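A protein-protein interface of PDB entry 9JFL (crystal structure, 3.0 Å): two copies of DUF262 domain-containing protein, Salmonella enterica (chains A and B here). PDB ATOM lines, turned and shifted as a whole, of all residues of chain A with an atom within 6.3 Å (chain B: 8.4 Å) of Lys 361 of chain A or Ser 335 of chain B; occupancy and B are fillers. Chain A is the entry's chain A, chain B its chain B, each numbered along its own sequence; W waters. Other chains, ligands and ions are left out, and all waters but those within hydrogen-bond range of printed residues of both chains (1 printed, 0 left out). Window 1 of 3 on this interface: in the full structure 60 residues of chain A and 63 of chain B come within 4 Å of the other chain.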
ATOM      1  N   LEU A 355     -11.855 -14.984 -10.878  1.00  0.00           N
ATOM      2  CA  LEU A 355     -11.879 -15.253  -9.442  1.00  0.00           C
ATOM      3  C   LEU A 355     -12.198 -16.719  -9.244  1.00  0.00           C
ATOM      4  O   LEU A 355     -11.449 -17.455  -8.607  1.00  0.00           O
ATOM      5  CB  LEU A 355     -12.943 -14.392  -8.749  1.00  0.00           C
ATOM      6  CG  LEU A 355     -13.288 -14.645  -7.271  1.00  0.00           C
ATOM      7  CD1 LEU A 355     -12.286 -13.992  -6.335  1.00  0.00           C
ATOM      8  CD2 LEU A 355     -14.666 -14.114  -6.959  1.00  0.00           C
ATOM      9  N   LEU A 356     -13.312 -17.139  -9.825  1.00  0.00           N
ATOM     10  CA  LEU A 356     -13.821 -18.488  -9.631  1.00  0.00           C
ATOM     11  C   LEU A 356     -12.789 -19.552 -10.023  1.00  0.00           C
ATOM     12  O   LEU A 356     -12.551 -20.482  -9.262  1.00  0.00           O
ATOM     13  CB  LEU A 356     -15.118 -18.678 -10.430  1.00  0.00           C
ATOM     14  CG  LEU A 356     -15.864 -19.999 -10.277  1.00  0.00           C
ATOM     15  CD1 LEU A 356     -16.180 -20.232  -8.820  1.00  0.00           C
ATOM     16  CD2 LEU A 356     -17.153 -20.033 -11.084  1.00  0.00           C
ATOM     17  N   ILE A 357     -12.164 -19.393 -11.190  1.00  0.00           N
ATOM     18  CA  ILE A 357     -11.322 -20.446 -11.760  1.00  0.00           C
ATOM     19  C   ILE A 357      -9.843 -20.295 -11.414  1.00  0.00           C
ATOM     20  O   ILE A 357      -9.218 -21.276 -10.987  1.00  0.00           O
ATOM     21  CB  ILE A 357     -11.511 -20.556 -13.292  1.00  0.00           C
ATOM     22  CG1 ILE A 357     -12.917 -21.071 -13.622  1.00  0.00           C
ATOM     23  CG2 ILE A 357     -10.475 -21.469 -13.913  1.00  0.00           C
ATOM     24  CD1 ILE A 357     -13.462 -22.098 -12.653  1.00  0.00           C
ATOM     25  N   ASN A 358      -9.285 -19.095 -11.598  1.00  0.00           N
ATOM     26  CA  ASN A 358      -7.849 -18.884 -11.367  1.00  0.00           C
ATOM     27  C   ASN A 358      -7.476 -18.587  -9.898  1.00  0.00           C
ATOM     28  O   ASN A 358      -6.398 -18.961  -9.458  1.00  0.00           O
ATOM     29  CB  ASN A 358      -7.300 -17.776 -12.271  1.00  0.00           C
ATOM     30  CG  ASN A 358      -7.406 -18.103 -13.756  1.00  0.00           C
ATOM     31  OD1 ASN A 358      -7.151 -19.224 -14.177  1.00  0.00           O
ATOM     32  ND2 ASN A 358      -7.754 -17.098 -14.561  1.00  0.00           N
ATOM     33  N   LYS A 359      -8.348 -17.928  -9.141  1.00  0.00           N
ATOM     34  CA  LYS A 359      -7.999 -17.493  -7.785  1.00  0.00           C
ATOM     35  C   LYS A 359      -8.494 -18.477  -6.745  1.00  0.00           C
ATOM     36  O   LYS A 359      -7.810 -18.743  -5.760  1.00  0.00           O
ATOM     37  CB  LYS A 359      -8.548 -16.083  -7.493  1.00  0.00           C
ATOM     38  CG  LYS A 359      -7.783 -15.357  -6.382  1.00  0.00           C
ATOM     39  CD  LYS A 359      -7.839 -13.824  -6.439  1.00  0.00           C
ATOM     40  CE  LYS A 359      -7.193 -13.242  -7.695  1.00  0.00           C
ATOM     41  NZ  LYS A 359      -5.748 -13.549  -7.867  1.00  0.00           N
ATOM     42  N   LEU A 360      -9.690 -19.006  -6.969  1.00  0.00           N
ATOM     43  CA  LEU A 360     -10.325 -19.949  -6.044  1.00  0.00           C
ATOM     44  C   LEU A 360     -10.319 -21.403  -6.549  1.00  0.00           C
ATOM     45  O   LEU A 360     -10.554 -22.320  -5.773  1.00  0.00           O
ATOM     46  CB  LEU A 360     -11.753 -19.485  -5.736  1.00  0.00           C
ATOM     47  CG  LEU A 360     -11.849 -18.022  -5.243  1.00  0.00           C
ATOM     48  CD1 LEU A 360     -13.289 -17.564  -5.102  1.00  0.00           C
ATOM     49  CD2 LEU A 360     -11.096 -17.782  -3.936  1.00  0.00           C
ATOM     50  N   LYS A 361     -10.067 -21.607  -7.848  1.00  0.00           N
ATOM     51  CA  LYS A 361      -9.706 -22.925  -8.380  1.00  0.00           C
ATOM     52  C   LYS A 361     -10.850 -23.966  -8.294  1.00  0.00           C
ATOM     53  O   LYS A 361     -10.648 -25.140  -8.000  1.00  0.00           O
ATOM     54  CB  LYS A 361      -8.419 -23.407  -7.689  1.00  0.00           C
ATOM     55  CG  LYS A 361      -7.288 -22.370  -7.697  1.00  0.00           C
ATOM     56  CD  LYS A 361      -5.995 -22.947  -7.127  1.00  0.00           C
ATOM     57  CE  LYS A 361      -4.735 -22.449  -7.823  1.00  0.00           C
ATOM     58  NZ  LYS A 361      -4.078 -21.350  -7.078  1.00  0.00           N
ATOM     59  N   HIS A 362     -12.055 -23.523  -8.586  1.00  0.00           N
ATOM     60  CA  HIS A 362     -13.238 -24.333  -8.389  1.00  0.00           C
ATOM     61  C   HIS A 362     -13.489 -25.016  -9.698  1.00  0.00           C
ATOM     62  O   HIS A 362     -14.447 -24.698 -10.429  1.00  0.00           O
ATOM     63  CB  HIS A 362     -14.415 -23.433  -7.986  1.00  0.00           C
ATOM     64  CG  HIS A 362     -15.675 -24.165  -7.656  1.00  0.00           C
ATOM     65  ND1 HIS A 362     -15.689 -25.343  -6.945  1.00  0.00           N
ATOM     66  CD2 HIS A 362     -16.969 -23.856  -7.905  1.00  0.00           C
ATOM     67  CE1 HIS A 362     -16.943 -25.737  -6.781  1.00  0.00           C
ATOM     68  NE2 HIS A 362     -17.737 -24.853  -7.355  1.00  0.00           N
ATOM     69  N   LEU A 363     -12.598 -25.953 -10.005  1.00  0.00           N
ATOM     70  CA  LEU A 363     -12.693 -26.672 -11.255  1.00  0.00           C
ATOM     71  C   LEU A 363     -13.993 -27.452 -11.283  1.00  0.00           C
ATOM     72  O   LEU A 363     -14.629 -27.532 -12.322  1.00  0.00           O
ATOM     73  CB  LEU A 363     -11.494 -27.570 -11.456  1.00  0.00           C
ATOM     74  CG  LEU A 363     -10.149 -26.837 -11.477  1.00  0.00           C
ATOM     75  CD1 LEU A 363      -9.042 -27.824 -11.814  1.00  0.00           C
ATOM     76  CD2 LEU A 363     -10.126 -25.667 -12.453  1.00  0.00           C
ATOM     77  N   HIS A 364     -14.444 -27.952 -10.131  1.00  0.00           N
ATOM     78  CA  HIS A 364     -15.705 -28.711 -10.073  1.00  0.00           C
ATOM     79  C   HIS A 364     -16.820 -28.127 -10.945  1.00  0.00           C
ATOM     80  O   HIS A 364     -17.704 -28.857 -11.420  1.00  0.00           O
ATOM     81  CB  HIS A 364     -16.213 -28.785  -8.642  1.00  0.00           C
ATOM     82  CG  HIS A 364     -15.697 -29.958  -7.881  1.00  0.00           C
ATOM     83  ND1 HIS A 364     -14.522 -29.919  -7.161  1.00  0.00           N
ATOM     84  CD2 HIS A 364     -16.201 -31.203  -7.717  1.00  0.00           C
ATOM     85  CE1 HIS A 364     -14.318 -31.093  -6.596  1.00  0.00           C
ATOM     86  NE2 HIS A 364     -15.324 -31.889  -6.914  1.00  0.00           N
ATOM     87  N   PHE A 391     -19.883 -20.957  -3.988  1.00  0.00           N
ATOM     88  CA  PHE A 391     -18.609 -21.548  -3.654  1.00  0.00           C
ATOM     89  C   PHE A 391     -17.956 -20.828  -2.492  1.00  0.00           C
ATOM     90  O   PHE A 391     -17.379 -21.442  -1.613  1.00  0.00           O
ATOM     91  CB  PHE A 391     -17.651 -21.513  -4.831  1.00  0.00           C
ATOM     92  CG  PHE A 391     -16.292 -22.044  -4.492  1.00  0.00           C
ATOM     93  CD1 PHE A 391     -16.078 -23.412  -4.388  1.00  0.00           C
ATOM     94  CD2 PHE A 391     -15.239 -21.185  -4.240  1.00  0.00           C
ATOM     95  CE1 PHE A 391     -14.838 -23.913  -4.065  1.00  0.00           C
ATOM     96  CE2 PHE A 391     -13.985 -21.685  -3.916  1.00  0.00           C
ATOM     97  CZ  PHE A 391     -13.784 -23.045  -3.827  1.00  0.00           C
ATOM     98  N   LYS A 462      -8.047 -14.462   1.433  1.00  0.00           N
ATOM     99  CA  LYS A 462      -9.107 -14.700   0.456  1.00  0.00           C
ATOM    100  C   LYS A 462     -10.509 -14.895   1.043  1.00  0.00           C
ATOM    101  O   LYS A 462     -11.495 -14.426   0.470  1.00  0.00           O
ATOM    102  CB  LYS A 462      -8.753 -15.925  -0.399  1.00  0.00           C
ATOM    103  CG  LYS A 462      -7.590 -15.722  -1.353  1.00  0.00           C
ATOM    104  CD  LYS A 462      -7.276 -17.022  -2.066  1.00  0.00           C
ATOM    105  CE  LYS A 462      -5.873 -16.990  -2.616  1.00  0.00           C
ATOM    106  NZ  LYS A 462      -5.705 -15.896  -3.600  1.00  0.00           N
ATOM    107  N   LYS B 276      -0.082 -33.157  -3.891  1.00  0.00           N
ATOM    108  CA  LYS B 276       0.633 -31.972  -3.396  1.00  0.00           C
ATOM    109  C   LYS B 276       1.912 -32.355  -2.632  1.00  0.00           C
ATOM    110  O   LYS B 276       2.967 -31.734  -2.809  1.00  0.00           O
ATOM    111  CB  LYS B 276      -0.308 -31.095  -2.529  1.00  0.00           C
ATOM    112  CG  LYS B 276      -0.183 -29.576  -2.745  1.00  0.00           C
ATOM    113  CD  LYS B 276      -0.883 -29.065  -4.017  1.00  0.00           C
ATOM    114  CE  LYS B 276      -0.014 -29.100  -5.284  1.00  0.00           C
ATOM    115  NZ  LYS B 276       0.377 -27.734  -5.747  1.00  0.00           N
ATOM    116  N   TYR B 280       5.484 -31.356  -3.933  1.00  0.00           N
ATOM    117  CA  TYR B 280       6.315 -30.544  -3.038  1.00  0.00           C
ATOM    118  C   TYR B 280       7.685 -31.196  -2.866  1.00  0.00           C
ATOM    119  O   TYR B 280       8.723 -30.570  -3.108  1.00  0.00           O
ATOM    120  CB  TYR B 280       5.647 -30.325  -1.663  1.00  0.00           C
ATOM    121  CG  TYR B 280       4.470 -29.363  -1.637  1.00  0.00           C
ATOM    122  CD1 TYR B 280       4.076 -28.674  -2.766  1.00  0.00           C
ATOM    123  CD2 TYR B 280       3.779 -29.120  -0.460  1.00  0.00           C
ATOM    124  CE1 TYR B 280       3.010 -27.802  -2.728  1.00  0.00           C
ATOM    125  CE2 TYR B 280       2.709 -28.244  -0.413  1.00  0.00           C
ATOM    126  CZ  TYR B 280       2.330 -27.589  -1.552  1.00  0.00           C
ATOM    127  OH  TYR B 280       1.269 -26.717  -1.571  1.00  0.00           O
ATOM    128  N   TRP B 283       9.848 -30.641  -5.836  1.00  0.00           N
ATOM    129  CA  TRP B 283      10.346 -29.281  -5.846  1.00  0.00           C
ATOM    130  C   TRP B 283      11.423 -29.099  -4.770  1.00  0.00           C
ATOM    131  O   TRP B 283      12.491 -28.538  -5.017  1.00  0.00           O
ATOM    132  CB  TRP B 283       9.192 -28.287  -5.670  1.00  0.00           C
ATOM    133  CG  TRP B 283       8.260 -28.183  -6.867  1.00  0.00           C
ATOM    134  CD1 TRP B 283       8.597 -28.298  -8.178  1.00  0.00           C
ATOM    135  CD2 TRP B 283       6.858 -27.891  -6.841  1.00  0.00           C
ATOM    136  NE1 TRP B 283       7.496 -28.118  -8.976  1.00  0.00           N
ATOM    137  CE2 TRP B 283       6.414 -27.858  -8.180  1.00  0.00           C
ATOM    138  CE3 TRP B 283       5.930 -27.651  -5.817  1.00  0.00           C
ATOM    139  CZ2 TRP B 283       5.078 -27.604  -8.521  1.00  0.00           C
ATOM    140  CZ3 TRP B 283       4.609 -27.399  -6.159  1.00  0.00           C
ATOM    141  CH2 TRP B 283       4.195 -27.385  -7.499  1.00  0.00           C
ATOM    142  N   ARG B 329       5.786 -23.378   3.613  1.00  0.00           N
ATOM    143  CA  ARG B 329       5.940 -22.244   2.703  1.00  0.00           C
ATOM    144  C   ARG B 329       5.267 -22.478   1.364  1.00  0.00           C
ATOM    145  O   ARG B 329       4.719 -21.558   0.747  1.00  0.00           O
ATOM    146  CB  ARG B 329       7.422 -21.993   2.398  1.00  0.00           C
ATOM    147  CG  ARG B 329       8.226 -21.467   3.562  1.00  0.00           C
ATOM    148  CD  ARG B 329       9.666 -21.919   3.464  1.00  0.00           C
ATOM    149  NE  ARG B 329      10.436 -21.465   4.615  1.00  0.00           N
ATOM    150  CZ  ARG B 329      11.197 -20.371   4.656  1.00  0.00           C
ATOM    151  NH1 ARG B 329      11.346 -19.565   3.598  1.00  0.00           N
ATOM    152  NH2 ARG B 329      11.834 -20.090   5.785  1.00  0.00           N
ATOM    153  N   LEU B 330       5.382 -23.706   0.877  1.00  0.00           N
ATOM    154  CA  LEU B 330       4.937 -24.033  -0.475  1.00  0.00           C
ATOM    155  C   LEU B 330       3.429 -23.925  -0.552  1.00  0.00           C
ATOM    156  O   LEU B 330       2.877 -23.587  -1.605  1.00  0.00           O
ATOM    157  CB  LEU B 330       5.399 -25.438  -0.887  1.00  0.00           C
ATOM    158  CG  LEU B 330       6.827 -25.508  -1.413  1.00  0.00           C
ATOM    159  CD1 LEU B 330       7.315 -26.938  -1.444  1.00  0.00           C
ATOM    160  CD2 LEU B 330       6.892 -24.920  -2.802  1.00  0.00           C
ATOM    161  N   GLU B 331       2.768 -24.198   0.571  1.00  0.00           N
ATOM    162  CA  GLU B 331       1.326 -23.986   0.666  1.00  0.00           C
ATOM    163  C   GLU B 331       0.953 -22.528   0.431  1.00  0.00           C
ATOM    164  O   GLU B 331      -0.154 -22.267  -0.016  1.00  0.00           O
ATOM    165  CB  GLU B 331       0.769 -24.483   1.996  1.00  0.00           C
ATOM    166  CG  GLU B 331       0.825 -26.000   2.142  1.00  0.00           C
ATOM    167  CD  GLU B 331      -0.316 -26.706   1.439  1.00  0.00           C
ATOM    168  OE1 GLU B 331      -1.415 -26.775   2.023  1.00  0.00           O
ATOM    169  OE2 GLU B 331      -0.115 -27.203   0.315  1.00  0.00           O
ATOM    170  N   TYR B 332       1.864 -21.589   0.695  1.00  0.00           N
ATOM    171  CA  TYR B 332       1.650 -20.188   0.294  1.00  0.00           C
ATOM    172  C   TYR B 332       2.005 -20.012  -1.165  1.00  0.00           C
ATOM    173  O   TYR B 332       1.168 -19.577  -1.965  1.00  0.00           O
ATOM    174  CB  TYR B 332       2.409 -19.198   1.205  1.00  0.00           C
ATOM    175  CG  TYR B 332       1.831 -19.253   2.594  1.00  0.00           C
ATOM    176  CD1 TYR B 332       2.272 -20.192   3.506  1.00  0.00           C
ATOM    177  CD2 TYR B 332       0.751 -18.456   2.950  1.00  0.00           C
ATOM    178  CE1 TYR B 332       1.694 -20.306   4.758  1.00  0.00           C
ATOM    179  CE2 TYR B 332       0.171 -18.557   4.201  1.00  0.00           C
ATOM    180  CZ  TYR B 332       0.652 -19.484   5.097  1.00  0.00           C
ATOM    181  OH  TYR B 332       0.079 -19.585   6.331  1.00  0.00           O
ATOM    182  N   ILE B 333       3.221 -20.402  -1.527  1.00  0.00           N
ATOM    183  CA  ILE B 333       3.743 -20.076  -2.853  1.00  0.00           C
ATOM    184  C   ILE B 333       3.060 -20.854  -3.995  1.00  0.00           C
ATOM    185  O   ILE B 333       2.979 -20.339  -5.101  1.00  0.00           O
ATOM    186  CB  ILE B 333       5.264 -20.276  -2.919  1.00  0.00           C
ATOM    187  CG1 ILE B 333       5.958 -19.538  -1.773  1.00  0.00           C
ATOM    188  CG2 ILE B 333       5.811 -19.755  -4.233  1.00  0.00           C
ATOM    189  CD1 ILE B 333       7.405 -19.939  -1.582  1.00  0.00           C
ATOM    190  N   SER B 334       2.566 -22.071  -3.729  1.00  0.00           N
ATOM    191  CA  SER B 334       1.818 -22.875  -4.721  1.00  0.00           C
ATOM    192  C   SER B 334       0.470 -22.282  -5.064  1.00  0.00           C
ATOM    193  O   SER B 334      -0.083 -22.593  -6.114  1.00  0.00           O
ATOM    194  CB  SER B 334       1.547 -24.275  -4.190  1.00  0.00           C
ATOM    195  OG  SER B 334       2.752 -24.974  -4.039  1.00  0.00           O
ATOM    196  N   SER B 335      -0.082 -21.483  -4.148  1.00  0.00           N
ATOM    197  CA  SER B 335      -1.376 -20.828  -4.346  1.00  0.00           C
ATOM    198  C   SER B 335      -1.210 -19.327  -4.575  1.00  0.00           C
ATOM    199  O   SER B 335      -2.184 -18.583  -4.515  1.00  0.00           O
ATOM    200  CB  SER B 335      -2.324 -21.098  -3.161  1.00  0.00           C
ATOM    201  OG  SER B 335      -2.164 -20.137  -2.122  1.00  0.00           O
ATOM    202  N   GLY B 336       0.021 -18.892  -4.818  1.00  0.00           N
ATOM    203  CA  GLY B 336       0.286 -17.562  -5.356  1.00  0.00           C
ATOM    204  C   GLY B 336       0.385 -16.535  -4.264  1.00  0.00           C
ATOM    205  O   GLY B 336       0.355 -15.326  -4.529  1.00  0.00           O
ATOM    206  N   GLU B 337       0.557 -17.020  -3.040  1.00  0.00           N
ATOM    207  CA  GLU B 337       0.457 -16.178  -1.876  1.00  0.00           C
ATOM    208  C   GLU B 337       1.791 -15.916  -1.173  1.00  0.00           C
ATOM    209  O   GLU B 337       2.708 -16.726  -1.196  1.00  0.00           O
ATOM    210  CB  GLU B 337      -0.553 -16.785  -0.919  1.00  0.00           C
ATOM    211  CG  GLU B 337      -1.951 -16.837  -1.512  1.00  0.00           C
ATOM    212  CD  GLU B 337      -2.969 -17.358  -0.526  1.00  0.00           C
ATOM    213  OE1 GLU B 337      -3.836 -18.160  -0.952  1.00  0.00           O
ATOM    214  OE2 GLU B 337      -2.892 -16.978   0.670  1.00  0.00           O
ATOM    215  N   TRP B 338       1.864 -14.761  -0.526  1.00  0.00           N
ATOM    216  CA  TRP B 338       3.091 -14.262   0.068  1.00  0.00           C
ATOM    217  C   TRP B 338       3.483 -15.133   1.265  1.00  0.00           C
ATOM    218  O   TRP B 338       2.667 -15.377   2.142  1.00  0.00           O
ATOM    219  CB  TRP B 338       2.895 -12.802   0.518  1.00  0.00           C
ATOM    220  CG  TRP B 338       4.159 -12.027   0.528  1.00  0.00           C
ATOM    221  CD1 TRP B 338       4.809 -11.530   1.609  1.00  0.00           C
ATOM    222  CD2 TRP B 338       4.956 -11.698  -0.606  1.00  0.00           C
ATOM    223  NE1 TRP B 338       5.962 -10.888   1.218  1.00  0.00           N
ATOM    224  CE2 TRP B 338       6.077 -10.983  -0.137  1.00  0.00           C
ATOM    225  CE3 TRP B 338       4.821 -11.923  -1.978  1.00  0.00           C
ATOM    226  CZ2 TRP B 338       7.054 -10.502  -0.976  1.00  0.00           C
ATOM    227  CZ3 TRP B 338       5.783 -11.438  -2.820  1.00  0.00           C
ATOM    228  CH2 TRP B 338       6.896 -10.734  -2.319  1.00  0.00           C
ATOM    229  N   LEU B 353       3.768 -12.263  -7.730  1.00  0.00           N
ATOM    230  CA  LEU B 353       3.658 -13.653  -7.317  1.00  0.00           C
ATOM    231  C   LEU B 353       2.300 -14.231  -7.694  1.00  0.00           C
ATOM    232  O   LEU B 353       2.203 -15.399  -8.077  1.00  0.00           O
ATOM    233  CB  LEU B 353       3.851 -13.780  -5.804  1.00  0.00           C
ATOM    234  CG  LEU B 353       3.832 -15.225  -5.294  1.00  0.00           C
ATOM    235  CD1 LEU B 353       5.128 -15.932  -5.654  1.00  0.00           C
ATOM    236  CD2 LEU B 353       3.600 -15.308  -3.799  1.00  0.00           C
ATOM    237  N   ASP B 354       1.249 -13.428  -7.551  1.00  0.00           N
ATOM    238  CA  ASP B 354      -0.091 -13.874  -7.915  1.00  0.00           C
ATOM    239  C   ASP B 354      -0.121 -14.043  -9.419  1.00  0.00           C
ATOM    240  O   ASP B 354      -0.505 -15.084  -9.927  1.00  0.00           O
ATOM    241  CB  ASP B 354      -1.168 -12.870  -7.483  1.00  0.00           C
ATOM    242  CG  ASP B 354      -2.580 -13.422  -7.657  1.00  0.00           C
ATOM    243  OD1 ASP B 354      -3.049 -14.118  -6.728  1.00  0.00           O
ATOM    244  OD2 ASP B 354      -3.223 -13.181  -8.706  1.00  0.00           O
ATOM    245  N   LEU B 355       0.299 -13.004 -10.124  1.00  0.00           N
ATOM    246  CA  LEU B 355       0.376 -13.049 -11.569  1.00  0.00           C
ATOM    247  C   LEU B 355       1.126 -14.301 -12.028  1.00  0.00           C
ATOM    248  O   LEU B 355       0.623 -15.091 -12.830  1.00  0.00           O
ATOM    249  CB  LEU B 355       1.087 -11.796 -12.093  1.00  0.00           C
ATOM    250  CG  LEU B 355       1.302 -11.742 -13.601  1.00  0.00           C
ATOM    251  CD1 LEU B 355      -0.023 -11.727 -14.335  1.00  0.00           C
ATOM    252  CD2 LEU B 355       2.124 -10.532 -13.990  1.00  0.00           C
ATOM    253  N   ILE B 357       2.020 -17.240 -10.918  1.00  0.00           N
ATOM    254  CA  ILE B 357       1.656 -18.638 -10.739  1.00  0.00           C
ATOM    255  C   ILE B 357       0.156 -18.905 -10.693  1.00  0.00           C
ATOM    256  O   ILE B 357      -0.270 -19.996 -11.089  1.00  0.00           O
ATOM    257  CB  ILE B 357       2.413 -19.280  -9.550  1.00  0.00           C
ATOM    258  CG1 ILE B 357       1.644 -19.170  -8.243  1.00  0.00           C
ATOM    259  CG2 ILE B 357       3.826 -18.719  -9.418  1.00  0.00           C
ATOM    260  CD1 ILE B 357       0.923 -20.457  -7.905  1.00  0.00           C
ATOM    261  N   ASN B 358      -0.646 -17.946 -10.227  1.00  0.00           N
ATOM    262  CA  ASN B 358      -2.108 -18.076 -10.361  1.00  0.00           C
ATOM    263  C   ASN B 358      -2.614 -17.723 -11.763  1.00  0.00           C
ATOM    264  O   ASN B 358      -3.587 -18.308 -12.222  1.00  0.00           O
ATOM    265  CB  ASN B 358      -2.871 -17.256  -9.321  1.00  0.00           C
ATOM    266  CG  ASN B 358      -2.548 -17.663  -7.880  1.00  0.00           C
ATOM    267  OD1 ASN B 358      -2.229 -18.808  -7.598  1.00  0.00           O
ATOM    268  ND2 ASN B 358      -2.664 -16.716  -6.957  1.00  0.00           N
ATOM    269  N   LYS B 359      -1.951 -16.806 -12.457  1.00  0.00           N
ATOM    270  CA  LYS B 359      -2.492 -16.299 -13.718  1.00  0.00           C
ATOM    271  C   LYS B 359      -1.845 -16.970 -14.930  1.00  0.00           C
ATOM    272  O   LYS B 359      -2.531 -17.339 -15.896  1.00  0.00           O
ATOM    273  CB  LYS B 359      -2.335 -14.776 -13.782  1.00  0.00           C
ATOM    274  CG  LYS B 359      -3.483 -14.056 -14.489  1.00  0.00           C
ATOM    275  CD  LYS B 359      -3.602 -12.583 -14.080  1.00  0.00           C
ATOM    276  CE  LYS B 359      -4.267 -12.401 -12.716  1.00  0.00           C
ATOM    277  NZ  LYS B 359      -5.746 -12.603 -12.749  1.00  0.00           N
ATOM    278  N   LYS B 361       0.481 -19.571 -14.350  1.00  0.00           N
ATOM    279  CA  LYS B 361       0.569 -20.963 -13.966  1.00  0.00           C
ATOM    280  C   LYS B 361       1.967 -21.491 -14.253  1.00  0.00           C
ATOM    281  O   LYS B 361       2.165 -22.647 -14.598  1.00  0.00           O
ATOM    282  CB  LYS B 361      -0.530 -21.762 -14.678  1.00  0.00           C
ATOM    283  CG  LYS B 361      -1.928 -21.162 -14.504  1.00  0.00           C
ATOM    284  CD  LYS B 361      -3.010 -21.923 -15.267  1.00  0.00           C
ATOM    285  CE  LYS B 361      -4.422 -21.486 -14.875  1.00  0.00           C
ATOM    286  NZ  LYS B 361      -4.807 -20.147 -15.416  1.00  0.00           N
ATOM    287  N   LEU B 363       4.519 -22.875 -12.816  1.00  0.00           N
ATOM    288  CA  LEU B 363       4.971 -23.646 -11.646  1.00  0.00           C
ATOM    289  C   LEU B 363       6.439 -24.062 -11.694  1.00  0.00           C
ATOM    290  O   LEU B 363       7.070 -24.270 -10.668  1.00  0.00           O
ATOM    291  CB  LEU B 363       4.101 -24.892 -11.471  1.00  0.00           C
ATOM    292  CG  LEU B 363       2.644 -24.675 -11.036  1.00  0.00           C
ATOM    293  CD1 LEU B 363       2.127 -25.955 -10.394  1.00  0.00           C
ATOM    294  CD2 LEU B 363       2.474 -23.498 -10.075  1.00  0.00           C
ATOM    295  N   MET B 366       9.004 -22.883  -9.107  1.00  0.00           N
ATOM    296  CA  MET B 366       8.799 -23.172  -7.705  1.00  0.00           C
ATOM    297  C   MET B 366      10.058 -23.404  -6.865  1.00  0.00           C
ATOM    298  O   MET B 366      10.190 -22.810  -5.805  1.00  0.00           O
ATOM    299  CB  MET B 366       7.865 -24.363  -7.568  1.00  0.00           C
ATOM    300  CG  MET B 366       6.418 -24.031  -7.872  1.00  0.00           C
ATOM    301  SD  MET B 366       5.587 -23.356  -6.429  1.00  0.00           S
ATOM    302  CE  MET B 366       5.291 -21.710  -7.050  1.00  0.00           C
HETATM  303  O   HOH W   1      -5.768 -14.426 -10.313  1.00  0.00           O
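Among the printed residues, pairs that only touch across the chains: Asn 358 of chain A with Asn 358 of chain B (3.8 Å) and Lys 361 of chain A with Ser 335 of chain B (3.9 Å).
Asn 358 of chain B touches its own counterpart, Asn 358 of chain A. Asn 358 of chain A touches Lys 361 of chain B, and with the chains exchanged Lys 361 of chain A touches Asn 358 of chain B.
Water W1 lies within hydrogen-bond range of the side-chain amino group of Lys 359 of chain A, the side-chain amino group of Lys 359 of chain B and the side-chain carboxylate of Asp 354 of chain B.
OG of Ser 335 of chain B is in hydrogen-bond range of OE1 of Glu 337 of chain B (2.8 Å). OD1 of Asp 354 of chain B sits at hydrogen-bond distance from ND2 of Asn 358 of chain B. The backbone carbonyl oxygen (O) of Leu 356 of chain A sits at hydrogen-bond distance from the backbone NH (N) of Lys 361 of chain A (3.1 Å). The backbone carbonyl oxygen (O) of Tyr 332 of chain B lies within hydrogen-bond range of the backbone NH (N) of Glu 337 of chain B (2.8 Å). The backbone carbonyl oxygen (O) of Tyr 332 of chain B lies within hydrogen-bond range of the side-chain hydroxyl (OG) of Ser 335 of chain B (3.4 Å). O of Asp 354 of chain B sits at hydrogen-bond distance from N of Lys 359 of chain B, 3.4 Å away.
OD2 of Asp 354 of chain B lies within salt-bridge range of NZ of Lys 359 of chain A, at 2.7 Å. The side-chain amino group of Lys 361 of chain A lies within hydrogen-bond range of the side-chain amide oxygen of Asn 358 of chain B, at 3.2 Å. OD1 of Asn 358 of chain A sits at hydrogen-bond distance from NZ of Lys 361 of chain B (2.8 Å). OE1 of Glu 337 of chain B lies within salt-bridge range of NZ of Lys 462 of chain A (3.95 Å).
Of the 12 printed residues of chain A, 4 touch a printed residue of chain B. Of the 22 printed residues of chain B, 5 touch a printed residue of chain A. Along chain B the printed residues that touch a printed residue of chain A span positions 335 to 361. Among the printed residues, 6 pairs touch across the chains. Among the printed residues, Asp or Glu carboxylates within 4 Å of a Lys or Arg side-chain nitrogen of the other chain: Lys 359 of chain A with Asp 354 of chain B (2.7 Å) and Lys 462 of chain A with Glu 337 of chain B (3.95 Å).
Of chain B, only Ser 335 and Asn 358 come within 4 Å of Lys 361 of chain A. Of the printed residues of chain A, Glu 337 of chain B touches Lys 462 (2.9 Å). Printed residues of chain A within 4 Å of Asn 358 of chain B: Asn 358 (3.8 Å) and Lys 361 (3.2 Å). The nearest residue of chain A that does not touch Ser 335 of chain B is Lys 462 of chain A (4.4 Å). The nearest printed residue of chain B that does not touch Lys 359 of chain A is Asn 358 of chain B (4.5 Å).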
